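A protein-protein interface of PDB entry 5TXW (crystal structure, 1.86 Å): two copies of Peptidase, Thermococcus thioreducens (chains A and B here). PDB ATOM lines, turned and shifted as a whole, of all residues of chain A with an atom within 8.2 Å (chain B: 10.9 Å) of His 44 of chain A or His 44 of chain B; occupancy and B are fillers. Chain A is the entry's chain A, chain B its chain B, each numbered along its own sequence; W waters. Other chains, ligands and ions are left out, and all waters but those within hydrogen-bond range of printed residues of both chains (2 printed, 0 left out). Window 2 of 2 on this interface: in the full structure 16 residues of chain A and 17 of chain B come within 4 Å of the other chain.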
ATOM      1  N   GLY A  10       4.200   7.448  12.352  1.00  0.00           N
ATOM      2  CA  GLY A  10       4.017   8.195  13.589  1.00  0.00           C
ATOM      3  C   GLY A  10       4.813   9.478  13.697  1.00  0.00           C
ATOM      4  O   GLY A  10       4.897  10.068  14.798  1.00  0.00           O
ATOM      5  N   PHE A  11       5.277   9.986  12.546  1.00  0.00           N
ATOM      6  CA  PHE A  11       5.904  11.303  12.477  1.00  0.00           C
ATOM      7  C   PHE A  11       4.879  12.370  12.786  1.00  0.00           C
ATOM      8  O   PHE A  11       3.672  12.132  12.642  1.00  0.00           O
ATOM      9  CB  PHE A  11       6.564  11.553  11.125  1.00  0.00           C
ATOM     10  CG  PHE A  11       5.616  11.516   9.955  1.00  0.00           C
ATOM     11  CD1 PHE A  11       5.045  12.674   9.486  1.00  0.00           C
ATOM     12  CD2 PHE A  11       5.446  10.356   9.220  1.00  0.00           C
ATOM     13  CE1 PHE A  11       4.217  12.666   8.375  1.00  0.00           C
ATOM     14  CE2 PHE A  11       4.566  10.324   8.153  1.00  0.00           C
ATOM     15  CZ  PHE A  11       4.008  11.500   7.687  1.00  0.00           C
ATOM     16  N   GLU A  12       5.343  13.460  13.391  1.00  0.00           N
ATOM     17  CA  GLU A  12       4.517  14.617  13.537  1.00  0.00           C
ATOM     18  C   GLU A  12       4.332  15.232  12.137  1.00  0.00           C
ATOM     19  O   GLU A  12       5.297  15.682  11.513  1.00  0.00           O
ATOM     20  CB  GLU A  12       5.185  15.616  14.481  1.00  0.00           C
ATOM     21  CG  GLU A  12       4.216  16.470  15.273  1.00  0.00           C
ATOM     22  CD  GLU A  12       3.513  17.496  14.403  1.00  0.00           C
ATOM     23  OE1 GLU A  12       4.097  17.916  13.370  1.00  0.00           O
ATOM     24  OE2 GLU A  12       2.365  17.857  14.744  1.00  0.00           O
ATOM     25  N   ASP A  13       3.103  15.205  11.638  1.00  0.00           N
ATOM     26  CA  ASP A  13       2.825  15.461  10.216  1.00  0.00           C
ATOM     27  C   ASP A  13       3.413  16.791   9.748  1.00  0.00           C
ATOM     28  O   ASP A  13       4.075  16.852   8.728  1.00  0.00           O
ATOM     29  CB  ASP A  13       1.312  15.466   9.964  1.00  0.00           C
ATOM     30  CG  ASP A  13       0.630  14.215  10.446  1.00  0.00           C
ATOM     31  OD1 ASP A  13       0.787  13.887  11.645  1.00  0.00           O
ATOM     32  OD2 ASP A  13      -0.113  13.576   9.666  1.00  0.00           O
ATOM     33  N   LEU A  14       3.167  17.873  10.468  1.00  0.00           N
ATOM     34  CA  LEU A  14       3.629  19.187  10.000  1.00  0.00           C
ATOM     35  C   LEU A  14       5.150  19.281   9.944  1.00  0.00           C
ATOM     36  O   LEU A  14       5.705  20.085   9.187  1.00  0.00           O
ATOM     37  CB  LEU A  14       3.115  20.294  10.919  1.00  0.00           C
ATOM     38  CG  LEU A  14       1.618  20.531  10.924  1.00  0.00           C
ATOM     39  CD1 LEU A  14       1.295  21.542  12.007  1.00  0.00           C
ATOM     40  CD2 LEU A  14       1.156  21.082   9.590  1.00  0.00           C
ATOM     41  N   THR A  41       2.739   6.989   7.490  1.00  0.00           N
ATOM     42  CA  THR A  41       1.587   7.766   7.915  1.00  0.00           C
ATOM     43  C   THR A  41       1.907   8.463   9.222  1.00  0.00           C
ATOM     44  O   THR A  41       2.401   7.831  10.149  1.00  0.00           O
ATOM     45  CB  THR A  41       0.388   6.815   8.093  1.00  0.00           C
ATOM     46  OG1 THR A  41       0.170   6.174   6.844  1.00  0.00           O
ATOM     47  CG2 THR A  41      -0.873   7.560   8.496  1.00  0.00           C
ATOM     48  N   GLY A  42       1.581   9.748   9.308  1.00  0.00           N
ATOM     49  CA  GLY A  42       1.842  10.535  10.501  1.00  0.00           C
ATOM     50  C   GLY A  42       0.814  10.343  11.595  1.00  0.00           C
ATOM     51  O   GLY A  42      -0.253   9.780  11.368  1.00  0.00           O
ATOM     52  N   LYS A  43       1.099  10.930  12.747  1.00  0.00           N
ATOM     53  CA  LYS A  43       0.172  10.947  13.870  1.00  0.00           C
ATOM     54  C   LYS A  43      -1.222  11.410  13.480  1.00  0.00           C
ATOM     55  O   LYS A  43      -2.206  10.977  14.090  1.00  0.00           O
ATOM     56  CB  LYS A  43       0.675  11.885  14.966  1.00  0.00           C
ATOM     57  CG  LYS A  43       1.897  11.379  15.708  1.00  0.00           C
ATOM     58  CD  LYS A  43       2.413  12.448  16.661  1.00  0.00           C
ATOM     59  CE  LYS A  43       1.443  12.694  17.807  1.00  0.00           C
ATOM     60  NZ  LYS A  43       2.158  13.325  18.945  1.00  0.00           N
ATOM     61  N   HIS A  44      -1.297  12.464  12.666  1.00  0.00           N
ATOM     62  CA  HIS A  44      -2.593  13.039  12.292  1.00  0.00           C
ATOM     63  C   HIS A  44      -3.165  12.509  10.991  1.00  0.00           C
ATOM     64  O   HIS A  44      -4.123  13.071  10.474  1.00  0.00           O
ATOM     65  CB  HIS A  44      -2.517  14.561  12.231  1.00  0.00           C
ATOM     66  CG  HIS A  44      -2.183  15.189  13.539  1.00  0.00           C
ATOM     67  ND1 HIS A  44      -3.115  15.858  14.302  1.00  0.00           N
ATOM     68  CD2 HIS A  44      -1.014  15.275  14.213  1.00  0.00           C
ATOM     69  CE1 HIS A  44      -2.557  16.235  15.438  1.00  0.00           C
ATOM     70  NE2 HIS A  44      -1.282  15.889  15.409  1.00  0.00           N
ATOM     71  N   GLY A  45      -2.533  11.495  10.413  1.00  0.00           N
ATOM     72  CA  GLY A  45      -3.162  10.732   9.341  1.00  0.00           C
ATOM     73  C   GLY A  45      -2.762  11.142   7.938  1.00  0.00           C
ATOM     74  O   GLY A  45      -3.141  10.473   6.982  1.00  0.00           O
ATOM     75  N   TYR A  46      -1.859  12.110   7.794  1.00  0.00           N
ATOM     76  CA  TYR A  46      -1.251  12.343   6.476  1.00  0.00           C
ATOM     77  C   TYR A  46      -0.251  11.251   6.094  1.00  0.00           C
ATOM     78  O   TYR A  46       0.452  10.707   6.943  1.00  0.00           O
ATOM     79  CB  TYR A  46      -0.567  13.700   6.416  1.00  0.00           C
ATOM     80  CG  TYR A  46      -1.519  14.866   6.394  1.00  0.00           C
ATOM     81  CD1 TYR A  46      -2.196  15.198   5.238  1.00  0.00           C
ATOM     82  CD2 TYR A  46      -1.690  15.679   7.508  1.00  0.00           C
ATOM     83  CE1 TYR A  46      -2.993  16.319   5.178  1.00  0.00           C
ATOM     84  CE2 TYR A  46      -2.457  16.829   7.441  1.00  0.00           C
ATOM     85  CZ  TYR A  46      -3.142  17.113   6.281  1.00  0.00           C
ATOM     86  OH  TYR A  46      -3.913  18.234   6.181  1.00  0.00           O
ATOM     87  N   SER A  47      -0.215  10.914   4.808  1.00  0.00           N
ATOM     88  CA  SER A  47       0.733   9.929   4.269  1.00  0.00           C
ATOM     89  C   SER A  47       1.783  10.560   3.369  1.00  0.00           C
ATOM     90  O   SER A  47       1.484  11.456   2.610  1.00  0.00           O
ATOM     91  CB  SER A  47      -0.010   8.882   3.455  1.00  0.00           C
ATOM     92  OG  SER A  47      -0.602   7.959   4.341  1.00  0.00           O
ATOM     93  N   PRO A 151       5.925  22.420  16.755  1.00  0.00           N
ATOM     94  CA  PRO A 151       5.450  22.924  15.476  1.00  0.00           C
ATOM     95  C   PRO A 151       5.240  24.442  15.428  1.00  0.00           C
ATOM     96  O   PRO A 151       5.321  25.034  14.360  1.00  0.00           O
ATOM     97  CB  PRO A 151       4.141  22.157  15.270  1.00  0.00           C
ATOM     98  CG  PRO A 151       4.353  20.873  16.008  1.00  0.00           C
ATOM     99  CD  PRO A 151       5.117  21.275  17.228  1.00  0.00           C
ATOM    100  N   ALA B   8     -12.320  28.446   8.397  1.00  0.00           N
ATOM    101  CA  ALA B   8     -13.308  28.006   9.395  1.00  0.00           C
ATOM    102  C   ALA B   8     -12.941  26.592   9.796  1.00  0.00           C
ATOM    103  O   ALA B   8     -12.035  26.011   9.197  1.00  0.00           O
ATOM    104  CB  ALA B   8     -14.733  28.061   8.808  1.00  0.00           C
ATOM    105  N   ASP B   9     -13.723  25.975  10.682  1.00  0.00           N
ATOM    106  CA  ASP B   9     -13.562  24.560  10.972  1.00  0.00           C
ATOM    107  C   ASP B   9     -13.620  23.737   9.698  1.00  0.00           C
ATOM    108  O   ASP B   9     -14.486  23.959   8.851  1.00  0.00           O
ATOM    109  CB  ASP B   9     -14.639  24.040  11.935  1.00  0.00           C
ATOM    110  CG  ASP B   9     -14.462  24.565  13.361  1.00  0.00           C
ATOM    111  OD1 ASP B   9     -13.333  24.705  13.821  1.00  0.00           O
ATOM    112  OD2 ASP B   9     -15.441  25.044  13.941  1.00  0.00           O
ATOM    113  N   GLY B  10     -12.857  22.651   9.697  1.00  0.00           N
ATOM    114  CA  GLY B  10     -12.823  21.714   8.586  1.00  0.00           C
ATOM    115  C   GLY B  10     -11.905  22.139   7.452  1.00  0.00           C
ATOM    116  O   GLY B  10     -11.899  21.527   6.384  1.00  0.00           O
ATOM    117  N   PHE B  11     -11.026  23.087   7.729  1.00  0.00           N
ATOM    118  CA  PHE B  11      -9.951  23.412   6.789  1.00  0.00           C
ATOM    119  C   PHE B  11      -8.995  22.258   6.569  1.00  0.00           C
ATOM    120  O   PHE B  11      -8.806  21.394   7.435  1.00  0.00           O
ATOM    121  CB  PHE B  11      -9.197  24.668   7.241  1.00  0.00           C
ATOM    122  CG  PHE B  11      -8.455  24.515   8.549  1.00  0.00           C
ATOM    123  CD1 PHE B  11      -7.114  24.156   8.564  1.00  0.00           C
ATOM    124  CD2 PHE B  11      -9.054  24.883   9.747  1.00  0.00           C
ATOM    125  CE1 PHE B  11      -6.423  24.018   9.771  1.00  0.00           C
ATOM    126  CE2 PHE B  11      -8.355  24.806  10.942  1.00  0.00           C
ATOM    127  CZ  PHE B  11      -7.041  24.379  10.952  1.00  0.00           C
ATOM    128  N   GLU B  12      -8.422  22.206   5.387  1.00  0.00           N
ATOM    129  CA  GLU B  12      -7.342  21.266   5.136  1.00  0.00           C
ATOM    130  C   GLU B  12      -6.059  21.746   5.821  1.00  0.00           C
ATOM    131  O   GLU B  12      -5.515  22.812   5.494  1.00  0.00           O
ATOM    132  CB  GLU B  12      -7.089  21.047   3.647  1.00  0.00           C
ATOM    133  CG  GLU B  12      -6.097  19.923   3.381  1.00  0.00           C
ATOM    134  CD  GLU B  12      -6.633  18.568   3.805  1.00  0.00           C
ATOM    135  OE1 GLU B  12      -6.143  18.003   4.801  1.00  0.00           O
ATOM    136  OE2 GLU B  12      -7.587  18.092   3.158  1.00  0.00           O
ATOM    137  N   ASP B  13      -5.618  20.981   6.816  1.00  0.00           N
ATOM    138  CA  ASP B  13      -4.736  21.524   7.846  1.00  0.00           C
ATOM    139  C   ASP B  13      -3.474  22.099   7.204  1.00  0.00           C
ATOM    140  O   ASP B  13      -2.997  23.150   7.592  1.00  0.00           O
ATOM    141  CB  ASP B  13      -4.359  20.426   8.852  1.00  0.00           C
ATOM    142  CG  ASP B  13      -5.558  19.795   9.495  1.00  0.00           C
ATOM    143  OD1 ASP B  13      -6.438  19.294   8.747  1.00  0.00           O
ATOM    144  OD2 ASP B  13      -5.578  19.723  10.749  1.00  0.00           O
ATOM    145  N   LEU B  14      -2.843  21.328   6.342  1.00  0.00           N
ATOM    146  CA  LEU B  14      -1.582  21.757   5.714  1.00  0.00           C
ATOM    147  C   LEU B  14      -1.743  23.038   4.878  1.00  0.00           C
ATOM    148  O   LEU B  14      -0.776  23.770   4.707  1.00  0.00           O
ATOM    149  CB  LEU B  14      -1.058  20.677   4.781  1.00  0.00           C
ATOM    150  CG  LEU B  14      -0.691  19.355   5.403  1.00  0.00           C
ATOM    151  CD1 LEU B  14      -0.331  18.389   4.290  1.00  0.00           C
ATOM    152  CD2 LEU B  14       0.450  19.550   6.387  1.00  0.00           C
ATOM    153  N   GLU B  15      -2.879  23.149   4.176  1.00  0.00           N
ATOM    154  CA  GLU B  15      -3.123  24.254   3.256  1.00  0.00           C
ATOM    155  C   GLU B  15      -3.222  25.572   3.994  1.00  0.00           C
ATOM    156  O   GLU B  15      -3.049  26.617   3.394  1.00  0.00           O
ATOM    157  CB  GLU B  15      -4.381  24.023   2.435  1.00  0.00           C
ATOM    158  CG  GLU B  15      -4.225  22.837   1.499  1.00  0.00           C
ATOM    159  CD  GLU B  15      -5.485  22.435   0.783  1.00  0.00           C
ATOM    160  OE1 GLU B  15      -6.537  23.105   0.937  1.00  0.00           O
ATOM    161  OE2 GLU B  15      -5.387  21.454   0.015  1.00  0.00           O
ATOM    162  N   LEU B  16      -3.532  25.528   5.288  1.00  0.00           N
ATOM    163  CA  LEU B  16      -3.558  26.744   6.094  1.00  0.00           C
ATOM    164  C   LEU B  16      -2.247  26.918   6.874  1.00  0.00           C
ATOM    165  O   LEU B  16      -1.628  28.000   6.871  1.00  0.00           O
ATOM    166  CB  LEU B  16      -4.758  26.675   7.050  1.00  0.00           C
ATOM    167  CG  LEU B  16      -4.907  27.737   8.137  1.00  0.00           C
ATOM    168  CD1 LEU B  16      -4.997  29.133   7.529  1.00  0.00           C
ATOM    169  CD2 LEU B  16      -6.122  27.437   9.009  1.00  0.00           C
ATOM    170  N   ILE B  17      -1.793  25.849   7.521  1.00  0.00           N
ATOM    171  CA  ILE B  17      -0.700  25.988   8.482  1.00  0.00           C
ATOM    172  C   ILE B  17       0.684  26.132   7.782  1.00  0.00           C
ATOM    173  O   ILE B  17       1.492  26.957   8.196  1.00  0.00           O
ATOM    174  CB  ILE B  17      -0.731  24.833   9.510  1.00  0.00           C
ATOM    175  CG1 ILE B  17      -1.986  24.951  10.383  1.00  0.00           C
ATOM    176  CG2 ILE B  17       0.484  24.880  10.428  1.00  0.00           C
ATOM    177  CD1 ILE B  17      -2.310  23.687  11.165  1.00  0.00           C
ATOM    178  N   ILE B  40     -10.095  27.400  15.502  1.00  0.00           N
ATOM    179  CA  ILE B  40     -10.798  26.513  14.580  1.00  0.00           C
ATOM    180  C   ILE B  40      -9.946  25.287  14.408  1.00  0.00           C
ATOM    181  O   ILE B  40      -8.724  25.353  14.561  1.00  0.00           O
ATOM    182  CB  ILE B  40     -11.003  27.201  13.211  1.00  0.00           C
ATOM    183  CG1 ILE B  40      -9.709  27.845  12.725  1.00  0.00           C
ATOM    184  CG2 ILE B  40     -12.049  28.298  13.314  1.00  0.00           C
ATOM    185  CD1 ILE B  40      -9.811  28.394  11.313  1.00  0.00           C
ATOM    186  N   THR B  41     -10.564  24.212  13.963  1.00  0.00           N
ATOM    187  CA  THR B  41      -9.929  22.912  13.939  1.00  0.00           C
ATOM    188  C   THR B  41     -10.081  22.262  12.576  1.00  0.00           C
ATOM    189  O   THR B  41     -11.145  22.364  11.965  1.00  0.00           O
ATOM    190  CB  THR B  41     -10.525  22.029  15.056  1.00  0.00           C
ATOM    191  OG1 THR B  41     -10.233  22.641  16.318  1.00  0.00           O
ATOM    192  CG2 THR B  41      -9.928  20.646  15.040  1.00  0.00           C
ATOM    193  N   GLY B  42      -8.938  21.839  12.023  1.00  0.00           N
ATOM    194  CA  GLY B  42      -8.836  21.280  10.684  1.00  0.00           C
ATOM    195  C   GLY B  42      -9.368  19.862  10.584  1.00  0.00           C
ATOM    196  O   GLY B  42      -9.608  19.211  11.597  1.00  0.00           O
ATOM    197  N   LYS B  43      -9.493  19.375   9.350  1.00  0.00           N
ATOM    198  CA  LYS B  43      -9.966  18.026   9.078  1.00  0.00           C
ATOM    199  C   LYS B  43      -9.155  17.036   9.877  1.00  0.00           C
ATOM    200  O   LYS B  43      -9.635  15.930  10.137  1.00  0.00           O
ATOM    201  CB  LYS B  43      -9.814  17.672   7.586  1.00  0.00           C
ATOM    202  CG  LYS B  43     -10.792  18.360   6.651  1.00  0.00           C
ATOM    203  CD  LYS B  43     -10.307  18.344   5.195  1.00  0.00           C
ATOM    204  CE  LYS B  43     -10.856  17.179   4.380  1.00  0.00           C
ATOM    205  NZ  LYS B  43      -9.828  16.117   4.219  1.00  0.00           N
ATOM    206  N   HIS B  44      -7.852  17.305  10.000  1.00  0.00           N
ATOM    207  CA  HIS B  44      -6.935  16.346  10.616  1.00  0.00           C
ATOM    208  C   HIS B  44      -6.626  16.638  12.067  1.00  0.00           C
ATOM    209  O   HIS B  44      -5.829  15.944  12.675  1.00  0.00           O
ATOM    210  CB  HIS B  44      -5.622  16.264   9.857  1.00  0.00           C
ATOM    211  CG  HIS B  44      -5.762  15.714   8.485  1.00  0.00           C
ATOM    212  ND1 HIS B  44      -5.487  14.399   8.186  1.00  0.00           N
ATOM    213  CD2 HIS B  44      -6.174  16.292   7.331  1.00  0.00           C
ATOM    214  CE1 HIS B  44      -5.696  14.195   6.896  1.00  0.00           C
ATOM    215  NE2 HIS B  44      -6.143  15.320   6.364  1.00  0.00           N
ATOM    216  N   GLY B  45      -7.266  17.634  12.643  1.00  0.00           N
ATOM    217  CA  GLY B  45      -7.215  17.790  14.096  1.00  0.00           C
ATOM    218  C   GLY B  45      -6.291  18.854  14.629  1.00  0.00           C
ATOM    219  O   GLY B  45      -6.264  19.086  15.828  1.00  0.00           O
ATOM    220  N   TYR B  46      -5.572  19.549  13.755  1.00  0.00           N
ATOM    221  CA  TYR B  46      -4.756  20.676  14.195  1.00  0.00           C
ATOM    222  C   TYR B  46      -5.653  21.857  14.455  1.00  0.00           C
ATOM    223  O   TYR B  46      -6.604  22.094  13.713  1.00  0.00           O
ATOM    224  CB  TYR B  46      -3.704  21.053  13.131  1.00  0.00           C
ATOM    225  CG  TYR B  46      -2.538  20.085  13.011  1.00  0.00           C
ATOM    226  CD1 TYR B  46      -1.523  20.059  13.971  1.00  0.00           C
ATOM    227  CD2 TYR B  46      -2.442  19.201  11.945  1.00  0.00           C
ATOM    228  CE1 TYR B  46      -0.464  19.159  13.878  1.00  0.00           C
ATOM    229  CE2 TYR B  46      -1.380  18.309  11.838  1.00  0.00           C
ATOM    230  CZ  TYR B  46      -0.359  18.344  12.776  1.00  0.00           C
ATOM    231  OH  TYR B  46       0.730  17.509  12.655  1.00  0.00           O
ATOM    232  N   SER B  47      -5.293  22.672  15.427  1.00  0.00           N
ATOM    233  CA  SER B  47      -6.073  23.865  15.704  1.00  0.00           C
ATOM    234  C   SER B  47      -5.264  25.098  15.432  1.00  0.00           C
ATOM    235  O   SER B  47      -4.067  25.112  15.602  1.00  0.00           O
ATOM    236  CB  SER B  47      -6.522  23.877  17.170  1.00  0.00           C
ATOM    237  OG  SER B  47      -7.531  22.905  17.403  1.00  0.00           O
ATOM    238  N   VAL B  48      -5.962  26.185  15.165  1.00  0.00           N
ATOM    239  CA  VAL B  48      -5.332  27.426  14.811  1.00  0.00           C
ATOM    240  C   VAL B  48      -6.169  28.507  15.474  1.00  0.00           C
ATOM    241  O   VAL B  48      -7.402  28.387  15.553  1.00  0.00           O
ATOM    242  CB  VAL B  48      -5.359  27.593  13.269  1.00  0.00           C
ATOM    243  CG1 VAL B  48      -5.308  29.050  12.868  1.00  0.00           C
ATOM    244  CG2 VAL B  48      -4.215  26.819  12.638  1.00  0.00           C
ATOM    245  N   GLY B  69      -8.211  25.346   1.452  1.00  0.00           N
ATOM    246  CA  GLY B  69      -9.282  24.429   1.066  1.00  0.00           C
ATOM    247  C   GLY B  69      -9.836  23.644   2.240  1.00  0.00           C
ATOM    248  O   GLY B  69      -9.775  24.084   3.373  1.00  0.00           O
ATOM    249  N   GLY B  70     -10.201  22.396   1.978  1.00  0.00           N
ATOM    250  CA  GLY B  70     -10.920  21.597   2.945  1.00  0.00           C
ATOM    251  C   GLY B  70     -12.406  21.803   2.738  1.00  0.00           C
ATOM    252  O   GLY B  70     -12.864  22.108   1.629  1.00  0.00           O
ATOM    253  N   ARG B  71     -13.153  21.627   3.812  1.00  0.00           N
ATOM    254  CA  ARG B  71     -14.609  21.726   3.794  1.00  0.00           C
ATOM    255  C   ARG B  71     -15.049  23.112   4.284  1.00  0.00           C
ATOM    256  O   ARG B  71     -16.180  23.542   4.028  1.00  0.00           O
ATOM    257  CB  ARG B  71     -15.233  20.631   4.675  1.00  0.00           C
ATOM    258  CG  ARG B  71     -14.969  19.208   4.174  1.00  0.00           C
ATOM    259  CD  ARG B  71     -15.087  19.060   2.649  1.00  0.00           C
ATOM    260  NE  ARG B  71     -14.649  17.746   2.154  1.00  0.00           N
ATOM    261  CZ  ARG B  71     -14.806  17.317   0.897  1.00  0.00           C
ATOM    262  NH1 ARG B  71     -15.327  18.112  -0.037  1.00  0.00           N
ATOM    263  NH2 ARG B  71     -14.437  16.082   0.569  1.00  0.00           N
ATOM    264  N   ALA B  72     -14.074  23.901   4.717  1.00  0.00           N
ATOM    265  CA  ALA B  72     -14.377  25.228   5.195  1.00  0.00           C
ATOM    266  C   ALA B  72     -14.956  26.188   4.140  1.00  0.00           C
ATOM    267  O   ALA B  72     -15.872  26.953   4.455  1.00  0.00           O
ATOM    268  CB  ALA B  72     -13.162  25.827   5.891  1.00  0.00           C
ATOM    269  N   OCS B 100      -7.258  24.126  -3.786  1.00  0.00           N
ATOM    270  CA  OCS B 100      -8.201  23.056  -3.461  1.00  0.00           C
ATOM    271  CB  OCS B 100      -7.772  22.495  -2.081  1.00  0.00           C
ATOM    272  SG  OCS B 100      -8.582  20.949  -1.623  1.00  0.00           S
ATOM    273  C   OCS B 100      -9.620  23.572  -3.582  1.00  0.00           C
ATOM    274  O   OCS B 100      -9.991  24.070  -4.656  1.00  0.00           O
ATOM    275  OD1 OCS B 100      -9.711  21.250  -0.720  1.00  0.00           O
ATOM    276  OD2 OCS B 100      -7.502  20.200  -0.854  1.00  0.00           O
ATOM    277  OD3 OCS B 100      -8.882  20.335  -2.901  1.00  0.00           O
ATOM    278  N   PRO B 151      -2.655  19.488  -1.701  1.00  0.00           N
ATOM    279  CA  PRO B 151      -1.505  19.625  -0.817  1.00  0.00           C
ATOM    280  C   PRO B 151      -0.144  19.239  -1.463  1.00  0.00           C
ATOM    281  O   PRO B 151       0.890  19.816  -1.109  1.00  0.00           O
ATOM    282  CB  PRO B 151      -1.859  18.702   0.365  1.00  0.00           C
ATOM    283  CG  PRO B 151      -3.344  18.638   0.343  1.00  0.00           C
ATOM    284  CD  PRO B 151      -3.674  18.602  -1.118  1.00  0.00           C
HETATM  285  O   HOH W   1      -5.943  14.398  15.285  1.00  0.00           O
HETATM  286  O   HOH W   2      -6.381  13.174  12.237  1.00  0.00           O
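The side-chain hydroxyl (OH) of Tyr 46 of chain A sits at hydrogen-bond distance from the backbone NH (N) of Leu 14 of chain B, 3.3 Å away. O of His 44 of chain A lies within hydrogen-bond range of ND1 of His 44 of chain B (3.0 Å). The side-chain hydroxyl of Tyr 46 of chain A is in hydrogen-bond range of the side-chain carboxylate of Glu 12 of chain B. The side-chain carboxylate (OE2) of Glu 12 of chain A sits at hydrogen-bond distance from the side-chain hydroxyl (OH) of Tyr 46 of chain B. OH of Tyr 46 of chain B lies close to N of Asp 13 of chain A (3.5 Å). N of Leu 14 of chain A is in hydrogen-bond range of OH of Tyr 46 of chain B, at 3.3 Å. The side-chain hydroxyl (OH) of Tyr 46 of chain A lies within hydrogen-bond range of the backbone NH (N) of Asp 13 of chain B (3.3 Å).
The side-chain carboxylate (OE1) of Glu 12 of chain A sits at hydrogen-bond distance from the backbone NH (N) of Leu 14 of chain A, 3.0 Å away. N of Gly 45 of chain A is in hydrogen-bond range of OD2 of Asp 13 of chain A (3.3 Å). N of Gly 45 of chain B sits at hydrogen-bond distance from OD2 of Asp 13 of chain B. A ring nitrogen (NE2) of His 44 of chain B sits close to the side-chain carboxylate (OE1) of Glu 12 of chain B, 3.1 Å away. The side-chain carboxylate (OD1) of Asp 13 of chain A sits at hydrogen-bond distance from the backbone NH (N) of His 44 of chain A, 2.7 Å away. The side-chain carboxylate (OD2) of Asp 13 of chain A lies within hydrogen-bond range of the backbone NH (N) of Tyr 46 of chain A (2.9 Å).
Among the printed residues, pairs that only touch across the chains: Leu 14 of chain A with Leu 14 of chain B, Leu 14 of chain A with Ile 17 of chain B, His 44 of chain A with Tyr 46 of chain B and Tyr 46 of chain A with His 44 of chain B.
Of the printed residues of chain B, Glu 12 of chain A touches Tyr 46 (2.7 Å). No residue of chain B comes within 4 Å of Lys 43 of chain A. His 44 of chain A touches just these residues of chain B: His 44 and Tyr 46. No residue of chain B comes within 4 Å of Gly 45 of chain A. Printed residues of chain B within 4 Å of Tyr 46 of chain A: Glu 12 (2.6 Å), Asp 13 (3.3 Å), Leu 14 (3.3 Å) and His 44 (3.2 Å). Of chain A, only His 44 and Tyr 46 come within 4 Å of His 44 of chain B. OCS 100 of chain B touches none of the printed residues of chain A. The nearest residue of chain A that does not touch His 44 of chain B is Gly 45 of chain A (4.3 Å). The nearest printed residue of chain A that does not touch Ile 17 of chain B is Pro 151 of chain A (6.2 Å).
Printed residues of chain A that touch a printed residue of chain B: Glu 12, Asp 13, Leu 14, His 44 and Tyr 46. Hydrophobic or aromatic side chains of chain A within 4 Å of the printed part of chain B: Leu 14, His 44 and Tyr 46. Of the 25 printed residues of chain B, 6 touch a printed residue of chain A. Hydrophobic or aromatic side chains of chain B that line the printed part of chain A: Leu 14, Ile 17, His 44 and Tyr 46.
Asp 13 of chain A touches Tyr 46 of chain B, and with the chains exchanged Tyr 46 of chain A touches Asp 13 of chain B. Leu 14 of chain B touches its own counterpart, Leu 14 of chain A. Leu 14 of chain A touches Tyr 46 of chain B, and with the chains exchanged Tyr 46 of chain A touches Leu 14 of chain B. His 44 of chain B touches its own counterpart, His 44 of chain A. 13 positions are printed for both chains. Of the 11 pairs that touch across the chains among the printed residues, 10 have their exchanged pair printed and touching as well.
Water W2 lies within hydrogen-bond range of the backbone carbonyl oxygen (O) of His 44 of chain B (2.9 Å) and the backbone carbonyl oxygen (O) of His 44 of chain A (2.9 Å). Water W1 bridges the backbone carbonyl oxygen of His 44 of chain B and a ring nitrogen (ND1) of His 44 of chain A.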
